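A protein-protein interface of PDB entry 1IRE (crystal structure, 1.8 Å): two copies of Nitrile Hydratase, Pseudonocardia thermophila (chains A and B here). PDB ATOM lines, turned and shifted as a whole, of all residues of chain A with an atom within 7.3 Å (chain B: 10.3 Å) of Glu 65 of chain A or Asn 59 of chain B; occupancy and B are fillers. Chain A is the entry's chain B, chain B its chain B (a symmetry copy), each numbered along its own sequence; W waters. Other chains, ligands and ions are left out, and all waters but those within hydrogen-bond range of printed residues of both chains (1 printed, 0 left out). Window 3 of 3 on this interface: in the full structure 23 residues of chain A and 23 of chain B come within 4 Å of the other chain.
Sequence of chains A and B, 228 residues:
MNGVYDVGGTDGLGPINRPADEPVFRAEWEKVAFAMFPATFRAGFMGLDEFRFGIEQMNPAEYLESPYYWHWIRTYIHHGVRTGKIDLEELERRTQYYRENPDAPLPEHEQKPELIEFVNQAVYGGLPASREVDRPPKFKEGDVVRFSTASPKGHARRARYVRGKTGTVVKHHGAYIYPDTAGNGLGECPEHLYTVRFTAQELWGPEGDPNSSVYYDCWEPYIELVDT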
ATOM      1  N   GLY A  12     -20.708  13.302   1.857  1.00  0.00           N
ATOM      2  CA  GLY A  12     -21.347  12.175   2.520  1.00  0.00           C
ATOM      3  C   GLY A  12     -21.080  11.891   3.985  1.00  0.00           C
ATOM      4  O   GLY A  12     -21.453  10.822   4.472  1.00  0.00           O
ATOM      5  N   LEU A  13     -20.459  12.829   4.695  1.00  0.00           N
ATOM      6  CA  LEU A  13     -20.168  12.626   6.112  1.00  0.00           C
ATOM      7  C   LEU A  13     -21.377  12.835   7.024  1.00  0.00           C
ATOM      8  O   LEU A  13     -21.342  12.488   8.206  1.00  0.00           O
ATOM      9  CB  LEU A  13     -18.972  13.483   6.546  1.00  0.00           C
ATOM     10  CG  LEU A  13     -17.611  12.774   6.493  1.00  0.00           C
ATOM     11  CD1 LEU A  13     -17.548  11.755   5.372  1.00  0.00           C
ATOM     12  CD2 LEU A  13     -16.495  13.790   6.366  1.00  0.00           C
ATOM     13  N   ASN A  59      -6.937   4.110  12.553  1.00  0.00           N
ATOM     14  CA  ASN A  59      -7.835   3.329  11.710  1.00  0.00           C
ATOM     15  C   ASN A  59      -8.887   4.392  11.352  1.00  0.00           C
ATOM     16  O   ASN A  59      -9.477   5.003  12.240  1.00  0.00           O
ATOM     17  CB  ASN A  59      -8.462   2.206  12.557  1.00  0.00           C
ATOM     18  CG  ASN A  59      -9.498   1.380  11.796  1.00  0.00           C
ATOM     19  OD1 ASN A  59      -9.607   0.171  12.003  1.00  0.00           O
ATOM     20  ND2 ASN A  59     -10.279   2.029  10.945  1.00  0.00           N
ATOM     21  N   PRO A  60      -9.093   4.658  10.051  1.00  0.00           N
ATOM     22  CA  PRO A  60     -10.061   5.656   9.580  1.00  0.00           C
ATOM     23  C   PRO A  60     -11.476   5.500  10.135  1.00  0.00           C
ATOM     24  O   PRO A  60     -12.110   6.490  10.509  1.00  0.00           O
ATOM     25  CB  PRO A  60     -10.027   5.474   8.062  1.00  0.00           C
ATOM     26  CG  PRO A  60      -8.632   5.020   7.813  1.00  0.00           C
ATOM     27  CD  PRO A  60      -8.420   4.012   8.911  1.00  0.00           C
ATOM     28  N   ALA A  61     -11.973   4.266  10.180  1.00  0.00           N
ATOM     29  CA  ALA A  61     -13.314   4.016  10.701  1.00  0.00           C
ATOM     30  C   ALA A  61     -13.380   4.417  12.177  1.00  0.00           C
ATOM     31  O   ALA A  61     -14.361   5.012  12.622  1.00  0.00           O
ATOM     32  CB  ALA A  61     -13.694   2.549  10.529  1.00  0.00           C
ATOM     33  N   GLU A  62     -12.322   4.110  12.923  1.00  0.00           N
ATOM     34  CA  GLU A  62     -12.267   4.461  14.337  1.00  0.00           C
ATOM     35  C   GLU A  62     -12.175   5.982  14.490  1.00  0.00           C
ATOM     36  O   GLU A  62     -12.860   6.573  15.320  1.00  0.00           O
ATOM     37  CB  GLU A  62     -11.069   3.794  15.017  1.00  0.00           C
ATOM     38  CG  GLU A  62     -11.088   3.925  16.537  1.00  0.00           C
ATOM     39  CD  GLU A  62      -9.871   3.315  17.196  1.00  0.00           C
ATOM     40  OE1 GLU A  62      -8.820   3.987  17.245  1.00  0.00           O
ATOM     41  OE2 GLU A  62      -9.964   2.165  17.671  1.00  0.00           O
ATOM     42  N   TYR A  63     -11.344   6.607  13.661  1.00  0.00           N
ATOM     43  CA  TYR A  63     -11.165   8.055  13.690  1.00  0.00           C
ATOM     44  C   TYR A  63     -12.468   8.819  13.460  1.00  0.00           C
ATOM     45  O   TYR A  63     -12.810   9.724  14.223  1.00  0.00           O
ATOM     46  CB  TYR A  63     -10.142   8.478  12.632  1.00  0.00           C
ATOM     47  CG  TYR A  63     -10.023   9.977  12.461  1.00  0.00           C
ATOM     48  CD1 TYR A  63     -10.713  10.637  11.444  1.00  0.00           C
ATOM     49  CD2 TYR A  63      -9.229  10.737  13.321  1.00  0.00           C
ATOM     50  CE1 TYR A  63     -10.617  12.014  11.287  1.00  0.00           C
ATOM     51  CE2 TYR A  63      -9.126  12.119  13.172  1.00  0.00           C
ATOM     52  CZ  TYR A  63      -9.825  12.747  12.152  1.00  0.00           C
ATOM     53  OH  TYR A  63      -9.733  14.109  11.990  1.00  0.00           O
ATOM     54  N   LEU A  64     -13.181   8.448  12.400  1.00  0.00           N
ATOM     55  CA  LEU A  64     -14.431   9.103  12.021  1.00  0.00           C
ATOM     56  C   LEU A  64     -15.578   9.074  13.026  1.00  0.00           C
ATOM     57  O   LEU A  64     -16.382  10.007  13.062  1.00  0.00           O
ATOM     58  CB  LEU A  64     -14.928   8.553  10.677  1.00  0.00           C
ATOM     59  CG  LEU A  64     -14.090   8.895   9.439  1.00  0.00           C
ATOM     60  CD1 LEU A  64     -14.575   8.109   8.237  1.00  0.00           C
ATOM     61  CD2 LEU A  64     -14.164  10.389   9.163  1.00  0.00           C
ATOM     62  N   GLU A  65     -15.651   8.035  13.856  1.00  0.00           N
ATOM     63  CA  GLU A  65     -16.757   7.934  14.806  1.00  0.00           C
ATOM     64  C   GLU A  65     -16.422   7.859  16.294  1.00  0.00           C
ATOM     65  O   GLU A  65     -17.324   7.745  17.126  1.00  0.00           O
ATOM     66  CB  GLU A  65     -17.667   6.763  14.422  1.00  0.00           C
ATOM     67  CG  GLU A  65     -18.260   6.894  13.029  1.00  0.00           C
ATOM     68  CD  GLU A  65     -19.338   5.869  12.734  1.00  0.00           C
ATOM     69  OE1 GLU A  65     -19.246   4.732  13.237  1.00  0.00           O
ATOM     70  OE2 GLU A  65     -20.276   6.206  11.988  1.00  0.00           O
ATOM     71  N   SER A  66     -15.142   7.929  16.640  1.00  0.00           N
ATOM     72  CA  SER A  66     -14.754   7.863  18.051  1.00  0.00           C
ATOM     73  C   SER A  66     -14.785   9.238  18.714  1.00  0.00           C
ATOM     74  O   SER A  66     -14.690  10.265  18.036  1.00  0.00           O
ATOM     75  CB  SER A  66     -13.352   7.257  18.190  1.00  0.00           C
ATOM     76  OG  SER A  66     -12.369   8.074  17.570  1.00  0.00           O
ATOM     77  N   PRO A  67     -14.985   9.280  20.046  1.00  0.00           N
ATOM     78  CA  PRO A  67     -15.011  10.567  20.748  1.00  0.00           C
ATOM     79  C   PRO A  67     -13.674  11.253  20.479  1.00  0.00           C
ATOM     80  O   PRO A  67     -12.635  10.590  20.435  1.00  0.00           O
ATOM     81  CB  PRO A  67     -15.128  10.148  22.210  1.00  0.00           C
ATOM     82  CG  PRO A  67     -15.964   8.905  22.123  1.00  0.00           C
ATOM     83  CD  PRO A  67     -15.343   8.176  20.954  1.00  0.00           C
ATOM     84  N   TYR A  68     -13.711  12.565  20.268  1.00  0.00           N
ATOM     85  CA  TYR A  68     -12.512  13.341  19.971  1.00  0.00           C
ATOM     86  C   TYR A  68     -11.262  13.007  20.784  1.00  0.00           C
ATOM     87  O   TYR A  68     -10.213  12.717  20.212  1.00  0.00           O
ATOM     88  CB  TYR A  68     -12.807  14.840  20.090  1.00  0.00           C
ATOM     89  CG  TYR A  68     -11.593  15.715  19.863  1.00  0.00           C
ATOM     90  CD1 TYR A  68     -11.113  15.951  18.576  1.00  0.00           C
ATOM     91  CD2 TYR A  68     -10.927  16.310  20.936  1.00  0.00           C
ATOM     92  CE1 TYR A  68     -10.003  16.759  18.363  1.00  0.00           C
ATOM     93  CE2 TYR A  68      -9.818  17.119  20.734  1.00  0.00           C
ATOM     94  CZ  TYR A  68      -9.364  17.343  19.446  1.00  0.00           C
ATOM     95  OH  TYR A  68      -8.290  18.170  19.241  1.00  0.00           O
ATOM     96  N   HIS A  71      -8.782  10.174  20.074  1.00  0.00           N
ATOM     97  CA  HIS A  71      -7.736  10.375  19.063  1.00  0.00           C
ATOM     98  C   HIS A  71      -6.428  10.712  19.777  1.00  0.00           C
ATOM     99  O   HIS A  71      -5.363  10.223  19.404  1.00  0.00           O
ATOM    100  CB  HIS A  71      -8.082  11.533  18.116  1.00  0.00           C
ATOM    101  CG  HIS A  71      -9.403  11.387  17.426  1.00  0.00           C
ATOM    102  ND1 HIS A  71      -9.910  12.356  16.587  1.00  0.00           N
ATOM    103  CD2 HIS A  71     -10.338  10.409  17.480  1.00  0.00           C
ATOM    104  CE1 HIS A  71     -11.102  11.983  16.157  1.00  0.00           C
ATOM    105  NE2 HIS A  71     -11.386  10.806  16.684  1.00  0.00           N
ATOM    106  N   MET B   1     -19.628  12.171  -6.389  1.00  0.00           N
ATOM    107  CA  MET B   1     -19.425  12.802  -5.052  1.00  0.00           C
ATOM    108  C   MET B   1     -18.019  12.511  -4.532  1.00  0.00           C
ATOM    109  O   MET B   1     -17.393  11.533  -4.940  1.00  0.00           O
ATOM    110  CB  MET B   1     -20.473  12.278  -4.060  1.00  0.00           C
ATOM    111  CG  MET B   1     -20.361  10.793  -3.734  1.00  0.00           C
ATOM    112  SD  MET B   1     -21.625  10.224  -2.573  1.00  0.00           S
ATOM    113  CE  MET B   1     -20.937  10.781  -1.015  1.00  0.00           C
ATOM    114  N   GLY B   3     -16.811  11.068  -2.094  1.00  0.00           N
ATOM    115  CA  GLY B   3     -16.995  10.113  -1.016  1.00  0.00           C
ATOM    116  C   GLY B   3     -15.731   9.380  -0.621  1.00  0.00           C
ATOM    117  O   GLY B   3     -14.787   9.276  -1.406  1.00  0.00           O
ATOM    118  N   VAL B   4     -15.712   8.879   0.610  1.00  0.00           N
ATOM    119  CA  VAL B   4     -14.569   8.130   1.119  1.00  0.00           C
ATOM    120  C   VAL B   4     -14.347   6.846   0.304  1.00  0.00           C
ATOM    121  O   VAL B   4     -13.216   6.368   0.196  1.00  0.00           O
ATOM    122  CB  VAL B   4     -14.752   7.784   2.620  1.00  0.00           C
ATOM    123  CG1 VAL B   4     -13.626   6.883   3.102  1.00  0.00           C
ATOM    124  CG2 VAL B   4     -14.776   9.064   3.451  1.00  0.00           C
ATOM    125  N   TYR B   5     -15.423   6.318  -0.289  1.00  0.00           N
ATOM    126  CA  TYR B   5     -15.374   5.088  -1.108  1.00  0.00           C
ATOM    127  C   TYR B   5     -14.331   5.188  -2.236  1.00  0.00           C
ATOM    128  O   TYR B   5     -13.827   4.176  -2.722  1.00  0.00           O
ATOM    129  CB  TYR B   5     -16.750   4.810  -1.736  1.00  0.00           C
ATOM    130  CG  TYR B   5     -17.004   5.626  -2.987  1.00  0.00           C
ATOM    131  CD1 TYR B   5     -16.709   5.106  -4.250  1.00  0.00           C
ATOM    132  CD2 TYR B   5     -17.442   6.949  -2.909  1.00  0.00           C
ATOM    133  CE1 TYR B   5     -16.828   5.879  -5.396  1.00  0.00           C
ATOM    134  CE2 TYR B   5     -17.566   7.734  -4.058  1.00  0.00           C
ATOM    135  CZ  TYR B   5     -17.254   7.192  -5.293  1.00  0.00           C
ATOM    136  OH  TYR B   5     -17.335   7.964  -6.428  1.00  0.00           O
ATOM    137  N   PHE B  53     -24.095   4.421  -6.925  1.00  0.00           N
ATOM    138  CA  PHE B  53     -24.346   5.648  -6.177  1.00  0.00           C
ATOM    139  C   PHE B  53     -24.940   5.369  -4.787  1.00  0.00           C
ATOM    140  O   PHE B  53     -24.595   6.043  -3.818  1.00  0.00           O
ATOM    141  CB  PHE B  53     -25.256   6.581  -6.985  1.00  0.00           C
ATOM    142  CG  PHE B  53     -25.371   7.973  -6.419  1.00  0.00           C
ATOM    143  CD1 PHE B  53     -24.287   8.579  -5.785  1.00  0.00           C
ATOM    144  CD2 PHE B  53     -26.565   8.677  -6.518  1.00  0.00           C
ATOM    145  CE1 PHE B  53     -24.394   9.866  -5.260  1.00  0.00           C
ATOM    146  CE2 PHE B  53     -26.682   9.962  -5.996  1.00  0.00           C
ATOM    147  CZ  PHE B  53     -25.594  10.557  -5.365  1.00  0.00           C
ATOM    148  N   GLY B  54     -25.819   4.371  -4.695  1.00  0.00           N
ATOM    149  CA  GLY B  54     -26.418   4.029  -3.414  1.00  0.00           C
ATOM    150  C   GLY B  54     -25.364   3.599  -2.408  1.00  0.00           C
ATOM    151  O   GLY B  54     -25.447   3.919  -1.217  1.00  0.00           O
ATOM    152  N   ILE B  55     -24.374   2.858  -2.893  1.00  0.00           N
ATOM    153  CA  ILE B  55     -23.272   2.382  -2.057  1.00  0.00           C
ATOM    154  C   ILE B  55     -22.359   3.548  -1.663  1.00  0.00           C
ATOM    155  O   ILE B  55     -21.907   3.636  -0.523  1.00  0.00           O
ATOM    156  CB  ILE B  55     -22.444   1.304  -2.792  1.00  0.00           C
ATOM    157  CG1 ILE B  55     -23.310   0.067  -3.045  1.00  0.00           C
ATOM    158  CG2 ILE B  55     -21.185   0.948  -1.992  1.00  0.00           C
ATOM    159  CD1 ILE B  55     -22.597  -1.042  -3.801  1.00  0.00           C
ATOM    160  N   GLU B  56     -22.131   4.465  -2.598  1.00  0.00           N
ATOM    161  CA  GLU B  56     -21.273   5.622  -2.343  1.00  0.00           C
ATOM    162  C   GLU B  56     -21.829   6.535  -1.251  1.00  0.00           C
ATOM    163  O   GLU B  56     -21.079   7.261  -0.604  1.00  0.00           O
ATOM    164  CB  GLU B  56     -21.064   6.405  -3.637  1.00  0.00           C
ATOM    165  CG  GLU B  56     -20.400   5.558  -4.714  1.00  0.00           C
ATOM    166  CD  GLU B  56     -20.518   6.135  -6.114  1.00  0.00           C
ATOM    167  OE1 GLU B  56     -21.160   7.192  -6.292  1.00  0.00           O
ATOM    168  OE2 GLU B  56     -19.977   5.509  -7.046  1.00  0.00           O
ATOM    169  N   GLN B  57     -23.143   6.475  -1.044  1.00  0.00           N
ATOM    170  CA  GLN B  57     -23.807   7.300  -0.039  1.00  0.00           C
ATOM    171  C   GLN B  57     -23.848   6.674   1.357  1.00  0.00           C
ATOM    172  O   GLN B  57     -24.428   7.245   2.283  1.00  0.00           O
ATOM    173  CB  GLN B  57     -25.216   7.652  -0.509  1.00  0.00           C
ATOM    174  CG  GLN B  57     -25.228   8.538  -1.745  1.00  0.00           C
ATOM    175  CD  GLN B  57     -26.614   8.733  -2.305  1.00  0.00           C
ATOM    176  OE1 GLN B  57     -27.406   9.501  -1.767  1.00  0.00           O
ATOM    177  NE2 GLN B  57     -26.919   8.032  -3.390  1.00  0.00           N
ATOM    178  N   MET B  58     -23.223   5.511   1.505  1.00  0.00           N
ATOM    179  CA  MET B  58     -23.182   4.826   2.794  1.00  0.00           C
ATOM    180  C   MET B  58     -22.364   5.600   3.816  1.00  0.00           C
ATOM    181  O   MET B  58     -21.573   6.480   3.462  1.00  0.00           O
ATOM    182  CB  MET B  58     -22.523   3.448   2.654  1.00  0.00           C
ATOM    183  CG  MET B  58     -23.384   2.352   2.062  1.00  0.00           C
ATOM    184  SD  MET B  58     -22.424   0.827   1.927  1.00  0.00           S
ATOM    185  CE  MET B  58     -22.158   0.433   3.662  1.00  0.00           C
ATOM    186  N   ASN B  59     -22.581   5.270   5.086  1.00  0.00           N
ATOM    187  CA  ASN B  59     -21.824   5.845   6.192  1.00  0.00           C
ATOM    188  C   ASN B  59     -20.419   5.301   5.889  1.00  0.00           C
ATOM    189  O   ASN B  59     -20.237   4.092   5.764  1.00  0.00           O
ATOM    190  CB  ASN B  59     -22.360   5.267   7.516  1.00  0.00           C
ATOM    191  CG  ASN B  59     -21.573   5.730   8.741  1.00  0.00           C
ATOM    192  OD1 ASN B  59     -22.147   5.938   9.810  1.00  0.00           O
ATOM    193  ND2 ASN B  59     -20.261   5.857   8.601  1.00  0.00           N
ATOM    194  N   PRO B  60     -19.425   6.189   5.718  1.00  0.00           N
ATOM    195  CA  PRO B  60     -18.043   5.797   5.417  1.00  0.00           C
ATOM    196  C   PRO B  60     -17.436   4.770   6.370  1.00  0.00           C
ATOM    197  O   PRO B  60     -16.766   3.831   5.930  1.00  0.00           O
ATOM    198  CB  PRO B  60     -17.292   7.129   5.469  1.00  0.00           C
ATOM    199  CG  PRO B  60     -18.327   8.110   5.045  1.00  0.00           C
ATOM    200  CD  PRO B  60     -19.538   7.654   5.814  1.00  0.00           C
ATOM    201  N   ALA B  61     -17.659   4.949   7.671  1.00  0.00           N
ATOM    202  CA  ALA B  61     -17.126   4.015   8.659  1.00  0.00           C
ATOM    203  C   ALA B  61     -17.735   2.627   8.442  1.00  0.00           C
ATOM    204  O   ALA B  61     -17.037   1.616   8.527  1.00  0.00           O
ATOM    205  CB  ALA B  61     -17.412   4.508  10.074  1.00  0.00           C
ATOM    206  N   GLU B  62     -19.029   2.588   8.138  1.00  0.00           N
ATOM    207  CA  GLU B  62     -19.709   1.322   7.891  1.00  0.00           C
ATOM    208  C   GLU B  62     -19.188   0.699   6.593  1.00  0.00           C
ATOM    209  O   GLU B  62     -18.916  -0.496   6.534  1.00  0.00           O
ATOM    210  CB  GLU B  62     -21.223   1.526   7.801  1.00  0.00           C
ATOM    211  CG  GLU B  62     -22.008   0.217   7.783  1.00  0.00           C
ATOM    212  CD  GLU B  62     -23.498   0.427   7.634  1.00  0.00           C
ATOM    213  OE1 GLU B  62     -23.963   0.613   6.491  1.00  0.00           O
ATOM    214  OE2 GLU B  62     -24.209   0.401   8.660  1.00  0.00           O
ATOM    215  N   TYR B  63     -19.026   1.528   5.566  1.00  0.00           N
ATOM    216  CA  TYR B  63     -18.527   1.072   4.272  1.00  0.00           C
ATOM    217  C   TYR B  63     -17.151   0.416   4.365  1.00  0.00           C
ATOM    218  O   TYR B  63     -16.941  -0.684   3.851  1.00  0.00           O
ATOM    219  CB  TYR B  63     -18.459   2.247   3.292  1.00  0.00           C
ATOM    220  CG  TYR B  63     -17.784   1.911   1.980  1.00  0.00           C
ATOM    221  CD1 TYR B  63     -16.438   2.211   1.772  1.00  0.00           C
ATOM    222  CD2 TYR B  63     -18.487   1.283   0.951  1.00  0.00           C
ATOM    223  CE1 TYR B  63     -15.808   1.897   0.575  1.00  0.00           C
ATOM    224  CE2 TYR B  63     -17.865   0.963  -0.253  1.00  0.00           C
ATOM    225  CZ  TYR B  63     -16.525   1.274  -0.431  1.00  0.00           C
ATOM    226  OH  TYR B  63     -15.897   0.967  -1.614  1.00  0.00           O
ATOM    227  N   LEU B  64     -16.219   1.106   5.017  1.00  0.00           N
ATOM    228  CA  LEU B  64     -14.843   0.636   5.162  1.00  0.00           C
ATOM    229  C   LEU B  64     -14.621  -0.689   5.884  1.00  0.00           C
ATOM    230  O   LEU B  64     -13.667  -1.404   5.569  1.00  0.00           O
ATOM    231  CB  LEU B  64     -13.982   1.719   5.826  1.00  0.00           C
ATOM    232  CG  LEU B  64     -13.719   2.988   5.007  1.00  0.00           C
ATOM    233  CD1 LEU B  64     -13.050   4.043   5.867  1.00  0.00           C
ATOM    234  CD2 LEU B  64     -12.853   2.656   3.802  1.00  0.00           C
ATOM    235  N   GLU B  65     -15.496  -1.039   6.824  1.00  0.00           N
ATOM    236  CA  GLU B  65     -15.303  -2.275   7.580  1.00  0.00           C
ATOM    237  C   GLU B  65     -16.409  -3.327   7.530  1.00  0.00           C
ATOM    238  O   GLU B  65     -16.298  -4.371   8.175  1.00  0.00           O
ATOM    239  CB  GLU B  65     -14.969  -1.946   9.038  1.00  0.00           C
ATOM    240  CG  GLU B  65     -13.713  -1.106   9.192  1.00  0.00           C
ATOM    241  CD  GLU B  65     -13.246  -0.976  10.629  1.00  0.00           C
ATOM    242  OE1 GLU B  65     -14.095  -0.948  11.541  1.00  0.00           O
ATOM    243  OE2 GLU B  65     -12.022  -0.895  10.841  1.00  0.00           O
ATOM    244  N   SER B  66     -17.467  -3.072   6.770  1.00  0.00           N
ATOM    245  CA  SER B  66     -18.561  -4.041   6.679  1.00  0.00           C
ATOM    246  C   SER B  66     -18.306  -5.089   5.597  1.00  0.00           C
ATOM    247  O   SER B  66     -17.537  -4.850   4.661  1.00  0.00           O
ATOM    248  CB  SER B  66     -19.887  -3.323   6.396  1.00  0.00           C
ATOM    249  OG  SER B  66     -19.863  -2.666   5.136  1.00  0.00           O
ATOM    250  N   TRP B  70     -22.842  -6.472   2.267  1.00  0.00           N
ATOM    251  CA  TRP B  70     -23.694  -5.594   3.061  1.00  0.00           C
ATOM    252  C   TRP B  70     -23.869  -4.274   2.286  1.00  0.00           C
ATOM    253  O   TRP B  70     -24.911  -3.626   2.383  1.00  0.00           O
ATOM    254  CB  TRP B  70     -23.106  -5.325   4.450  1.00  0.00           C
ATOM    255  CG  TRP B  70     -23.899  -4.288   5.198  1.00  0.00           C
ATOM    256  CD1 TRP B  70     -23.510  -3.011   5.496  1.00  0.00           C
ATOM    257  CD2 TRP B  70     -25.259  -4.405   5.633  1.00  0.00           C
ATOM    258  NE1 TRP B  70     -24.552  -2.321   6.070  1.00  0.00           N
ATOM    259  CE2 TRP B  70     -25.636  -3.152   6.166  1.00  0.00           C
ATOM    260  CE3 TRP B  70     -26.199  -5.446   5.616  1.00  0.00           C
ATOM    261  CZ2 TRP B  70     -26.913  -2.911   6.680  1.00  0.00           C
ATOM    262  CZ3 TRP B  70     -27.472  -5.206   6.129  1.00  0.00           C
ATOM    263  CH2 TRP B  70     -27.816  -3.947   6.653  1.00  0.00           C
ATOM    264  N   HIS B  71     -22.852  -3.890   1.514  1.00  0.00           N
ATOM    265  CA  HIS B  71     -22.924  -2.665   0.707  1.00  0.00           C
ATOM    266  C   HIS B  71     -24.090  -2.795  -0.270  1.00  0.00           C
ATOM    267  O   HIS B  71     -24.841  -1.844  -0.486  1.00  0.00           O
ATOM    268  CB  HIS B  71     -21.637  -2.446  -0.103  1.00  0.00           C
ATOM    269  CG  HIS B  71     -20.391  -2.409   0.727  1.00  0.00           C
ATOM    270  ND1 HIS B  71     -19.137  -2.283   0.169  1.00  0.00           N
ATOM    271  CD2 HIS B  71     -20.200  -2.521   2.062  1.00  0.00           C
ATOM    272  CE1 HIS B  71     -18.226  -2.323   1.126  1.00  0.00           C
ATOM    273  NE2 HIS B  71     -18.845  -2.467   2.284  1.00  0.00           N
ATOM    274  N   ARG B  74     -27.384  -2.252   1.450  1.00  0.00           N
ATOM    275  CA  ARG B  74     -27.599  -0.825   1.677  1.00  0.00           C
ATOM    276  C   ARG B  74     -28.154  -0.116   0.444  1.00  0.00           C
ATOM    277  O   ARG B  74     -29.063   0.703   0.563  1.00  0.00           O
ATOM    278  CB  ARG B  74     -26.307  -0.133   2.132  1.00  0.00           C
ATOM    279  CG  ARG B  74     -25.995  -0.287   3.618  1.00  0.00           C
ATOM    280  CD  ARG B  74     -27.065   0.386   4.475  1.00  0.00           C
ATOM    281  NE  ARG B  74     -26.647   0.540   5.868  1.00  0.00           N
ATOM    282  CZ  ARG B  74     -27.466   0.847   6.867  1.00  0.00           C
ATOM    283  NH1 ARG B  74     -28.761   1.032   6.637  1.00  0.00           N
ATOM    284  NH2 ARG B  74     -26.989   0.992   8.097  1.00  0.00           N
ATOM    285  N   THR B  75     -27.633  -0.447  -0.737  1.00  0.00           N
ATOM    286  CA  THR B  75     -28.111   0.195  -1.959  1.00  0.00           C
ATOM    287  C   THR B  75     -29.530  -0.255  -2.340  1.00  0.00           C
ATOM    288  O   THR B  75     -30.297   0.529  -2.899  1.00  0.00           O
ATOM    289  CB  THR B  75     -27.115   0.033  -3.140  1.00  0.00           C
ATOM    290  OG1 THR B  75     -27.393   1.026  -4.130  1.00  0.00           O
ATOM    291  CG2 THR B  75     -27.223  -1.341  -3.779  1.00  0.00           C
ATOM    292  N   HIS B  78     -31.705   1.710   0.016  1.00  0.00           N
ATOM    293  CA  HIS B  78     -31.652   3.106  -0.409  1.00  0.00           C
ATOM    294  C   HIS B  78     -32.629   3.378  -1.556  1.00  0.00           C
ATOM    295  O   HIS B  78     -33.460   4.285  -1.478  1.00  0.00           O
ATOM    296  CB  HIS B  78     -30.227   3.469  -0.842  1.00  0.00           C
ATOM    297  CG  HIS B  78     -30.119   4.812  -1.495  1.00  0.00           C
ATOM    298  ND1 HIS B  78     -30.002   5.981  -0.775  1.00  0.00           N
ATOM    299  CD2 HIS B  78     -30.140   5.173  -2.799  1.00  0.00           C
ATOM    300  CE1 HIS B  78     -29.957   7.006  -1.611  1.00  0.00           C
ATOM    301  NE2 HIS B  78     -30.039   6.541  -2.844  1.00  0.00           N
HETATM  302  O   HOH W   1     -23.583   9.643   3.045  1.00  0.00           O
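Among the printed residues, pairs that only touch across the chains: Ala 61 of chain A with Glu 65 of chain B, Glu 65 of chain A with Ala 61 of chain B, Leu 13 of chain A with Pro 60 of chain B, Gly 12 of chain A with Met 1 of chain B and Gly 12 of chain A with Pro 60 of chain B.
The side-chain carboxylate (OE2) of Glu 65 of chain B sits close to the side-chain amide oxygen (OD1) of Asn 59 of chain A (2.9 Å). The side-chain amide oxygen (OD1) of Asn 59 of chain B sits close to the side-chain carboxylate (OE2) of Glu 65 of chain A, at 2.9 Å.
ND2 of Asn 59 of chain A sits close to N of Ala 61 of chain A. The side-chain amide nitrogen (ND2) of Asn 59 of chain B lies close to the backbone NH (N) of Ala 61 of chain B, at 2.9 Å.
Hydrophobic or aromatic side chains of chain B within 4 Å of the printed part of chain A: Met 1, Pro 60 and Ala 61. Along chain B the printed residues that touch a printed residue of chain A span positions 1 to 65. Of the 13 printed residues of chain A, 5 touch a printed residue of chain B. Printed residues of chain A that touch a printed residue of chain B: Gly 12, Leu 13, Asn 59, Ala 61 and Glu 65. Hydrophobic or aromatic side chains of chain A within 4 Å of the printed part of chain B: Leu 13 and Ala 61. Along chain A the printed residues that touch a printed residue of chain B span positions 12 to 65.
Water W1 lies within hydrogen-bond range of O of Gln 57 of chain B (2.7 Å) and O of Gly 12 of chain A (2.8 Å).
Glu 65 of chain A touches two residues of chain B. No residue of chain B comes within 4 Å of Pro 67 of chain A. Printed residues of chain B within 4 Å of Ala 61 of chain A: Glu 65 (3.6 Å). Of the printed residues of chain A, Ala 61 of chain B touches Glu 65. Printed residues of chain A within 4 Å of Met 1 of chain B: Gly 12. Phe 53 of chain B touches none of the printed residues of chain A. Glu 56 of chain B touches none of the printed residues of chain A. The nearest residue of chain A that does not touch Asn 59 of chain B is Gly 12 of chain A (5.3 Å).
Asn 59 of chain A touches Glu 65 of chain B, and with the chains exchanged Glu 65 of chain A touches Asn 59 of chain B. Ala 61 of chain A touches Glu 65 of chain B, and with the chains exchanged Glu 65 of chain A touches Ala 61 of chain B. 9 positions are printed for both chains. Of the 7 pairs that touch across the chains among the printed residues, 4 have their exchanged pair printed and touching as well.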
